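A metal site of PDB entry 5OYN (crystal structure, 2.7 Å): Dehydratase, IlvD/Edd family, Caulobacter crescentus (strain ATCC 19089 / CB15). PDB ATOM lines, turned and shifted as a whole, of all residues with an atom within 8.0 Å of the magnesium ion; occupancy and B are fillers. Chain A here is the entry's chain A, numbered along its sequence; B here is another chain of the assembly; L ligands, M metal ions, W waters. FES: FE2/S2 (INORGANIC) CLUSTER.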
ATOM      1  N   GLU A 101      14.589 -32.939 -24.635  1.00  0.00           N
ATOM      2  CA  GLU A 101      13.837 -31.709 -24.814  1.00  0.00           C
ATOM      3  C   GLU A 101      12.747 -31.518 -23.746  1.00  0.00           C
ATOM      4  O   GLU A 101      12.502 -30.407 -23.287  1.00  0.00           O
ATOM      5  CB  GLU A 101      13.224 -31.677 -26.212  1.00  0.00           C
ATOM      6  CG  GLU A 101      12.260 -30.522 -26.440  1.00  0.00           C
ATOM      7  CD  GLU A 101      12.870 -29.388 -27.263  1.00  0.00           C
ATOM      8  OE1 GLU A 101      12.081 -28.546 -27.766  1.00  0.00           O
ATOM      9  OE2 GLU A 101      14.132 -29.348 -27.389  1.00  0.00           O
ATOM     10  N   ASN A 102      12.095 -32.617 -23.333  1.00  0.00           N
ATOM     11  CA  ASN A 102      10.928 -32.479 -22.467  1.00  0.00           C
ATOM     12  C   ASN A 102      11.298 -31.887 -21.102  1.00  0.00           C
ATOM     13  O   ASN A 102      10.536 -31.066 -20.555  1.00  0.00           O
ATOM     14  CB  ASN A 102      10.225 -33.822 -22.298  1.00  0.00           C
ATOM     15  CG  ASN A 102       9.103 -34.040 -23.293  1.00  0.00           C
ATOM     16  OD1 ASN A 102       8.921 -33.283 -24.251  1.00  0.00           O
ATOM     17  ND2 ASN A 102       8.346 -35.106 -23.072  1.00  0.00           N
ATOM     18  N   THR A 107      15.502 -24.354 -21.513  1.00  0.00           N
ATOM     19  CA  THR A 107      15.052 -24.983 -22.749  1.00  0.00           C
ATOM     20  C   THR A 107      16.199 -25.801 -23.317  1.00  0.00           C
ATOM     21  O   THR A 107      17.371 -25.508 -23.074  1.00  0.00           O
ATOM     22  CB  THR A 107      14.574 -23.956 -23.796  1.00  0.00           C
ATOM     23  OG1 THR A 107      14.380 -24.609 -25.065  1.00  0.00           O
ATOM     24  CG2 THR A 107      15.586 -22.856 -23.965  1.00  0.00           C
ATOM     25  N   ALA A 108      15.853 -26.843 -24.077  1.00  0.00           N
ATOM     26  CA  ALA A 108      16.864 -27.675 -24.726  1.00  0.00           C
ATOM     27  C   ALA A 108      17.499 -26.992 -25.934  1.00  0.00           C
ATOM     28  O   ALA A 108      18.511 -27.500 -26.434  1.00  0.00           O
ATOM     29  CB  ALA A 108      16.275 -29.014 -25.137  1.00  0.00           C
ATOM     30  N   ALA A 109      16.937 -25.867 -26.414  1.00  0.00           N
ATOM     31  CA  ALA A 109      17.590 -25.132 -27.489  1.00  0.00           C
ATOM     32  C   ALA A 109      18.980 -24.686 -27.092  1.00  0.00           C
ATOM     33  O   ALA A 109      19.851 -24.495 -27.963  1.00  0.00           O
ATOM     34  CB  ALA A 109      16.744 -23.925 -27.891  1.00  0.00           C
ATOM     35  N   CYS A 137      15.734 -37.444 -30.316  1.00  0.00           N
ATOM     36  CA  CYS A 137      15.138 -36.269 -29.712  1.00  0.00           C
ATOM     37  C   CYS A 137      15.474 -35.027 -30.523  1.00  0.00           C
ATOM     38  O   CYS A 137      16.530 -34.955 -31.160  1.00  0.00           O
ATOM     39  CB  CYS A 137      15.651 -36.076 -28.279  1.00  0.00           C
ATOM     40  SG  CYS A 137      14.592 -34.994 -27.261  1.00  0.00           S
ATOM     41  N   ASP A 138      14.554 -34.051 -30.486  1.00  0.00           N
ATOM     42  CA  ASP A 138      14.523 -32.923 -31.428  1.00  0.00           C
ATOM     43  C   ASP A 138      15.880 -32.387 -31.905  1.00  0.00           C
ATOM     44  O   ASP A 138      16.139 -32.361 -33.103  1.00  0.00           O
ATOM     45  CB  ASP A 138      13.734 -31.726 -30.828  1.00  0.00           C
ATOM     46  CG  ASP A 138      12.368 -32.116 -30.293  1.00  0.00           C
ATOM     47  OD1 ASP A 138      11.726 -33.003 -30.939  1.00  0.00           O
ATOM     48  OD2 ASP A 138      11.882 -31.459 -29.324  1.00  0.00           O
ATOM     49  N   KCX A 139      16.753 -32.019 -30.974  1.00  0.00           N
ATOM     50  CA  KCX A 139      17.944 -31.259 -31.307  1.00  0.00           C
ATOM     51  CB  KCX A 139      18.194 -30.233 -30.207  1.00  0.00           C
ATOM     52  CG  KCX A 139      17.397 -28.979 -30.432  1.00  0.00           C
ATOM     53  CD  KCX A 139      16.693 -28.490 -29.201  1.00  0.00           C
ATOM     54  CE  KCX A 139      15.728 -27.384 -29.591  1.00  0.00           C
ATOM     55  NZ  KCX A 139      14.333 -27.913 -29.607  1.00  0.00           N
ATOM     56  C   KCX A 139      19.210 -32.059 -31.528  1.00  0.00           C
ATOM     57  O   KCX A 139      20.289 -31.483 -31.667  1.00  0.00           O
ATOM     58  CX  KCX A 139      13.655 -28.192 -30.722  1.00  0.00           C
ATOM     59  OQ1 KCX A 139      12.487 -28.642 -30.657  1.00  0.00           O
ATOM     60  OQ2 KCX A 139      14.189 -27.981 -31.844  1.00  0.00           O
ATOM     61  N   CYS A 210       9.045 -38.650 -29.936  1.00  0.00           N
ATOM     62  CA  CYS A 210       7.641 -38.248 -30.066  1.00  0.00           C
ATOM     63  C   CYS A 210       7.031 -38.861 -31.323  1.00  0.00           C
ATOM     64  O   CYS A 210       7.668 -38.873 -32.384  1.00  0.00           O
ATOM     65  CB  CYS A 210       7.538 -36.726 -30.094  1.00  0.00           C
ATOM     66  SG  CYS A 210       7.950 -35.983 -28.477  1.00  0.00           S
ATOM     67  N   GLY A 214       6.302 -34.103 -35.093  1.00  0.00           N
ATOM     68  CA  GLY A 214       6.933 -32.992 -34.410  1.00  0.00           C
ATOM     69  C   GLY A 214       8.339 -32.785 -34.911  1.00  0.00           C
ATOM     70  O   GLY A 214       8.713 -33.197 -36.015  1.00  0.00           O
ATOM     71  N   THR A 215       9.161 -32.133 -34.073  1.00  0.00           N
ATOM     72  CA  THR A 215      10.501 -31.772 -34.515  1.00  0.00           C
ATOM     73  C   THR A 215      11.350 -33.005 -34.777  1.00  0.00           C
ATOM     74  O   THR A 215      12.119 -33.038 -35.745  1.00  0.00           O
ATOM     75  CB  THR A 215      11.191 -30.870 -33.487  1.00  0.00           C
ATOM     76  OG1 THR A 215      10.282 -29.865 -33.058  1.00  0.00           O
ATOM     77  CG2 THR A 215      12.430 -30.237 -34.093  1.00  0.00           C
ATOM     78  N   ALA A 216      11.204 -34.039 -33.922  1.00  0.00           N
ATOM     79  CA  ALA A 216      12.025 -35.234 -34.033  1.00  0.00           C
ATOM     80  C   ALA A 216      11.693 -36.009 -35.303  1.00  0.00           C
ATOM     81  O   ALA A 216      12.589 -36.378 -36.067  1.00  0.00           O
ATOM     82  CB  ALA A 216      11.857 -36.121 -32.802  1.00  0.00           C
ATOM     83  N   SER A 286       7.516 -29.554 -38.614  1.00  0.00           N
ATOM     84  CA  SER A 286       7.564 -28.597 -37.523  1.00  0.00           C
ATOM     85  C   SER A 286       8.305 -27.320 -37.910  1.00  0.00           C
ATOM     86  O   SER A 286       9.327 -27.352 -38.608  1.00  0.00           O
ATOM     87  CB  SER A 286       8.252 -29.241 -36.322  1.00  0.00           C
ATOM     88  OG  SER A 286       8.961 -28.276 -35.562  1.00  0.00           O
ATOM     89  N   ASN A 288      10.161 -25.817 -36.090  1.00  0.00           N
ATOM     90  CA  ASN A 288      11.528 -25.850 -35.586  1.00  0.00           C
ATOM     91  C   ASN A 288      12.492 -26.335 -36.641  1.00  0.00           C
ATOM     92  O   ASN A 288      13.700 -26.103 -36.511  1.00  0.00           O
ATOM     93  CB  ASN A 288      11.590 -26.712 -34.336  1.00  0.00           C
ATOM     94  CG  ASN A 288      10.858 -26.093 -33.185  1.00  0.00           C
ATOM     95  OD1 ASN A 288      10.792 -24.870 -33.072  1.00  0.00           O
ATOM     96  ND2 ASN A 288      10.306 -26.913 -32.311  1.00  0.00           N
ATOM     97  N   HIS A 292      16.757 -25.051 -37.768  1.00  0.00           N
ATOM     98  CA  HIS A 292      17.709 -26.155 -37.857  1.00  0.00           C
ATOM     99  C   HIS A 292      18.217 -26.342 -39.268  1.00  0.00           C
ATOM    100  O   HIS A 292      19.398 -26.630 -39.463  1.00  0.00           O
ATOM    101  CB  HIS A 292      17.080 -27.460 -37.373  1.00  0.00           C
ATOM    102  CG  HIS A 292      16.754 -27.464 -35.919  1.00  0.00           C
ATOM    103  ND1 HIS A 292      17.603 -26.933 -34.969  1.00  0.00           N
ATOM    104  CD2 HIS A 292      15.669 -27.913 -35.255  1.00  0.00           C
ATOM    105  CE1 HIS A 292      17.058 -27.071 -33.774  1.00  0.00           C
ATOM    106  NE2 HIS A 292      15.879 -27.660 -33.914  1.00  0.00           N
ATOM    107  N   GLU A 472       9.785 -22.924 -26.505  1.00  0.00           N
ATOM    108  CA  GLU A 472       8.538 -23.392 -27.105  1.00  0.00           C
ATOM    109  C   GLU A 472       7.376 -22.899 -26.258  1.00  0.00           C
ATOM    110  O   GLU A 472       6.782 -23.650 -25.482  1.00  0.00           O
ATOM    111  CB  GLU A 472       8.511 -24.916 -27.220  1.00  0.00           C
ATOM    112  CG  GLU A 472       9.535 -25.524 -28.193  1.00  0.00           C
ATOM    113  CD  GLU A 472       9.535 -27.061 -28.215  1.00  0.00           C
ATOM    114  OE1 GLU A 472       8.915 -27.737 -27.352  1.00  0.00           O
ATOM    115  OE2 GLU A 472      10.224 -27.611 -29.141  1.00  0.00           O
ATOM    116  N   ARG A 497       9.474 -20.000 -29.950  1.00  0.00           N
ATOM    117  CA  ARG A 497       9.103 -21.161 -30.761  1.00  0.00           C
ATOM    118  C   ARG A 497       7.874 -21.838 -30.168  1.00  0.00           C
ATOM    119  O   ARG A 497       7.285 -21.349 -29.200  1.00  0.00           O
ATOM    120  CB  ARG A 497      10.282 -22.141 -30.860  1.00  0.00           C
ATOM    121  CG  ARG A 497      11.670 -21.464 -30.955  1.00  0.00           C
ATOM    122  CD  ARG A 497      12.799 -22.417 -31.298  1.00  0.00           C
ATOM    123  NE  ARG A 497      12.513 -23.766 -30.828  1.00  0.00           N
ATOM    124  CZ  ARG A 497      12.803 -24.208 -29.610  1.00  0.00           C
ATOM    125  NH1 ARG A 497      13.426 -23.418 -28.743  1.00  0.00           N
ATOM    126  NH2 ARG A 497      12.486 -25.444 -29.262  1.00  0.00           N
ATOM    127  N   GLN A 498       7.461 -22.942 -30.770  1.00  0.00           N
ATOM    128  CA  GLN A 498       6.442 -23.808 -30.193  1.00  0.00           C
ATOM    129  C   GLN A 498       6.815 -25.232 -30.528  1.00  0.00           C
ATOM    130  O   GLN A 498       7.577 -25.487 -31.460  1.00  0.00           O
ATOM    131  CB  GLN A 498       5.047 -23.489 -30.730  1.00  0.00           C
ATOM    132  CG  GLN A 498       4.803 -24.038 -32.116  1.00  0.00           C
ATOM    133  CD  GLN A 498       3.477 -23.600 -32.676  1.00  0.00           C
ATOM    134  OE1 GLN A 498       2.723 -22.854 -32.034  1.00  0.00           O
ATOM    135  NE2 GLN A 498       3.173 -24.058 -33.889  1.00  0.00           N
ATOM    136  N   SER A 499       6.280 -26.179 -29.751  1.00  0.00           N
ATOM    137  CA  SER A 499       6.599 -27.580 -29.992  1.00  0.00           C
ATOM    138  C   SER A 499       6.186 -27.998 -31.402  1.00  0.00           C
ATOM    139  O   SER A 499       5.118 -27.604 -31.889  1.00  0.00           O
ATOM    140  CB  SER A 499       5.914 -28.476 -28.967  1.00  0.00           C
ATOM    141  OG  SER A 499       6.264 -29.849 -29.155  1.00  0.00           O
ATOM    142  N   GLY A 500       7.036 -28.785 -32.048  1.00  0.00           N
ATOM    143  CA  GLY A 500       6.686 -29.322 -33.351  1.00  0.00           C
ATOM    144  C   GLY A 500       5.395 -30.104 -33.329  1.00  0.00           C
ATOM    145  O   GLY A 500       4.836 -30.465 -34.370  1.00  0.00           O
ATOM    146  N   THR A 501       4.918 -30.382 -32.137  1.00  0.00           N
ATOM    147  CA  THR A 501       3.675 -31.092 -31.901  1.00  0.00           C
ATOM    148  C   THR A 501       2.498 -30.144 -31.715  1.00  0.00           C
ATOM    149  O   THR A 501       1.385 -30.600 -31.438  1.00  0.00           O
ATOM    150  CB  THR A 501       3.826 -31.998 -30.670  1.00  0.00           C
ATOM    151  OG1 THR A 501       4.029 -31.186 -29.509  1.00  0.00           O
ATOM    152  CG2 THR A 501       5.048 -32.874 -30.848  1.00  0.00           C
ATOM    153  N   ASN B 599       9.999 -24.827 -19.526  1.00  0.00           N
ATOM    154  CA  ASN B 599      10.389 -24.822 -20.934  1.00  0.00           C
ATOM    155  C   ASN B 599       9.209 -24.889 -21.900  1.00  0.00           C
ATOM    156  O   ASN B 599       9.427 -24.835 -23.119  1.00  0.00           O
ATOM    157  CB  ASN B 599      11.346 -25.986 -21.225  1.00  0.00           C
ATOM    158  CG  ASN B 599      10.780 -27.343 -20.843  1.00  0.00           C
ATOM    159  OD1 ASN B 599       9.588 -27.490 -20.564  1.00  0.00           O
ATOM    160  ND2 ASN B 599      11.642 -28.343 -20.829  1.00  0.00           N
ATOM    161  N   HIS B 600       7.975 -25.001 -21.404  1.00  0.00           N
ATOM    162  CA  HIS B 600       6.782 -24.935 -22.249  1.00  0.00           C
ATOM    163  C   HIS B 600       5.692 -24.111 -21.568  1.00  0.00           C
ATOM    164  O   HIS B 600       5.966 -23.280 -20.702  1.00  0.00           O
ATOM    165  CB  HIS B 600       6.262 -26.346 -22.569  1.00  0.00           C
ATOM    166  CG  HIS B 600       7.129 -27.134 -23.495  1.00  0.00           C
ATOM    167  ND1 HIS B 600       8.316 -27.729 -23.081  1.00  0.00           N
ATOM    168  CD2 HIS B 600       6.979 -27.461 -24.798  1.00  0.00           C
ATOM    169  CE1 HIS B 600       8.852 -28.368 -24.102  1.00  0.00           C
ATOM    170  NE2 HIS B 600       8.063 -28.231 -25.154  1.00  0.00           N
ATOM    171  OXT HIS B 600       4.498 -24.259 -21.857  1.00  0.00           O
HETATM  172 FE1  FES L   1      12.581 -36.148 -27.217  1.00  0.00          FE
HETATM  173 FE2  FES L   1       9.931 -34.849 -27.974  1.00  0.00          FE
HETATM  174  S1  FES L   1      10.922 -35.280 -26.054  1.00  0.00           S
HETATM  175  S2  FES L   1      11.326 -36.197 -29.027  1.00  0.00           S
HETATM  176 MG    MG M   1      11.104 -29.501 -29.339  1.00  0.00          MG
HETATM  177  O   HOH W   1       9.387 -29.992 -30.560  1.00  0.00           O
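OD1 of Asn 102 lies close to S1 of the ligand, at 3.4 Å. The side-chain sulfur (SG) of Cys 137 binds an iron atom (FE1) of the ligand (2.3 Å). N of Cys 210 lies close to S2 of the ligand (3.5 Å). An iron atom (FE2) of the ligand is bound by the side-chain sulfur (SG) of Cys 210 (2.3 Å).
The side-chain carboxylate (OE1) of Glu 101 sits close to the guanidinium group (NH2) of Arg 497 (3.5 Å). N of Glu 101 lies close to SG of Cys 137, 3.3 Å away. The backbone carbonyl oxygen of Glu 101 lies within hydrogen-bond range of the side-chain amide nitrogen of Asn 599 of chain B (3.3 Å). OE2 of Glu 472 sits close to NH2 of Arg 497, 3.1 Å away. OQ1 of KCX 139 sits close to the side-chain hydroxyl (OG1) of Thr 215 (3.5 Å). The guanidinium group (NH2) of Arg 497 lies within salt-bridge range of OQ2 of KCX 139. OQ2 of KCX 139 is in hydrogen-bond range of a ring nitrogen (NE2) of His 292, 2.7 Å away. OD1 of Asp 138 is in hydrogen-bond range of N of Ala 216.
OG1 of Thr 215 touches the magnesium ion, at 3.8 Å.
The side-chain carboxylate (OE1) of Glu 101 is bound to the magnesium ion (2.1 Å). The magnesium ion is bound by the side-chain carboxylate (OE2) of Glu 472. OQ1 of KCX 139 binds the magnesium ion (2.1 Å). The side-chain carboxylate (OD2) of Asp 138 is bound to the magnesium ion, at 2.1 Å. Water W1 binds the magnesium ion, 2.2 Å away.
Water W1 lies within hydrogen-bond range of the side-chain hydroxyl (OG1) of Thr 215, the backbone NH (N) of Gly 500 and the side-chain hydroxyl (OG) of Ser 499.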
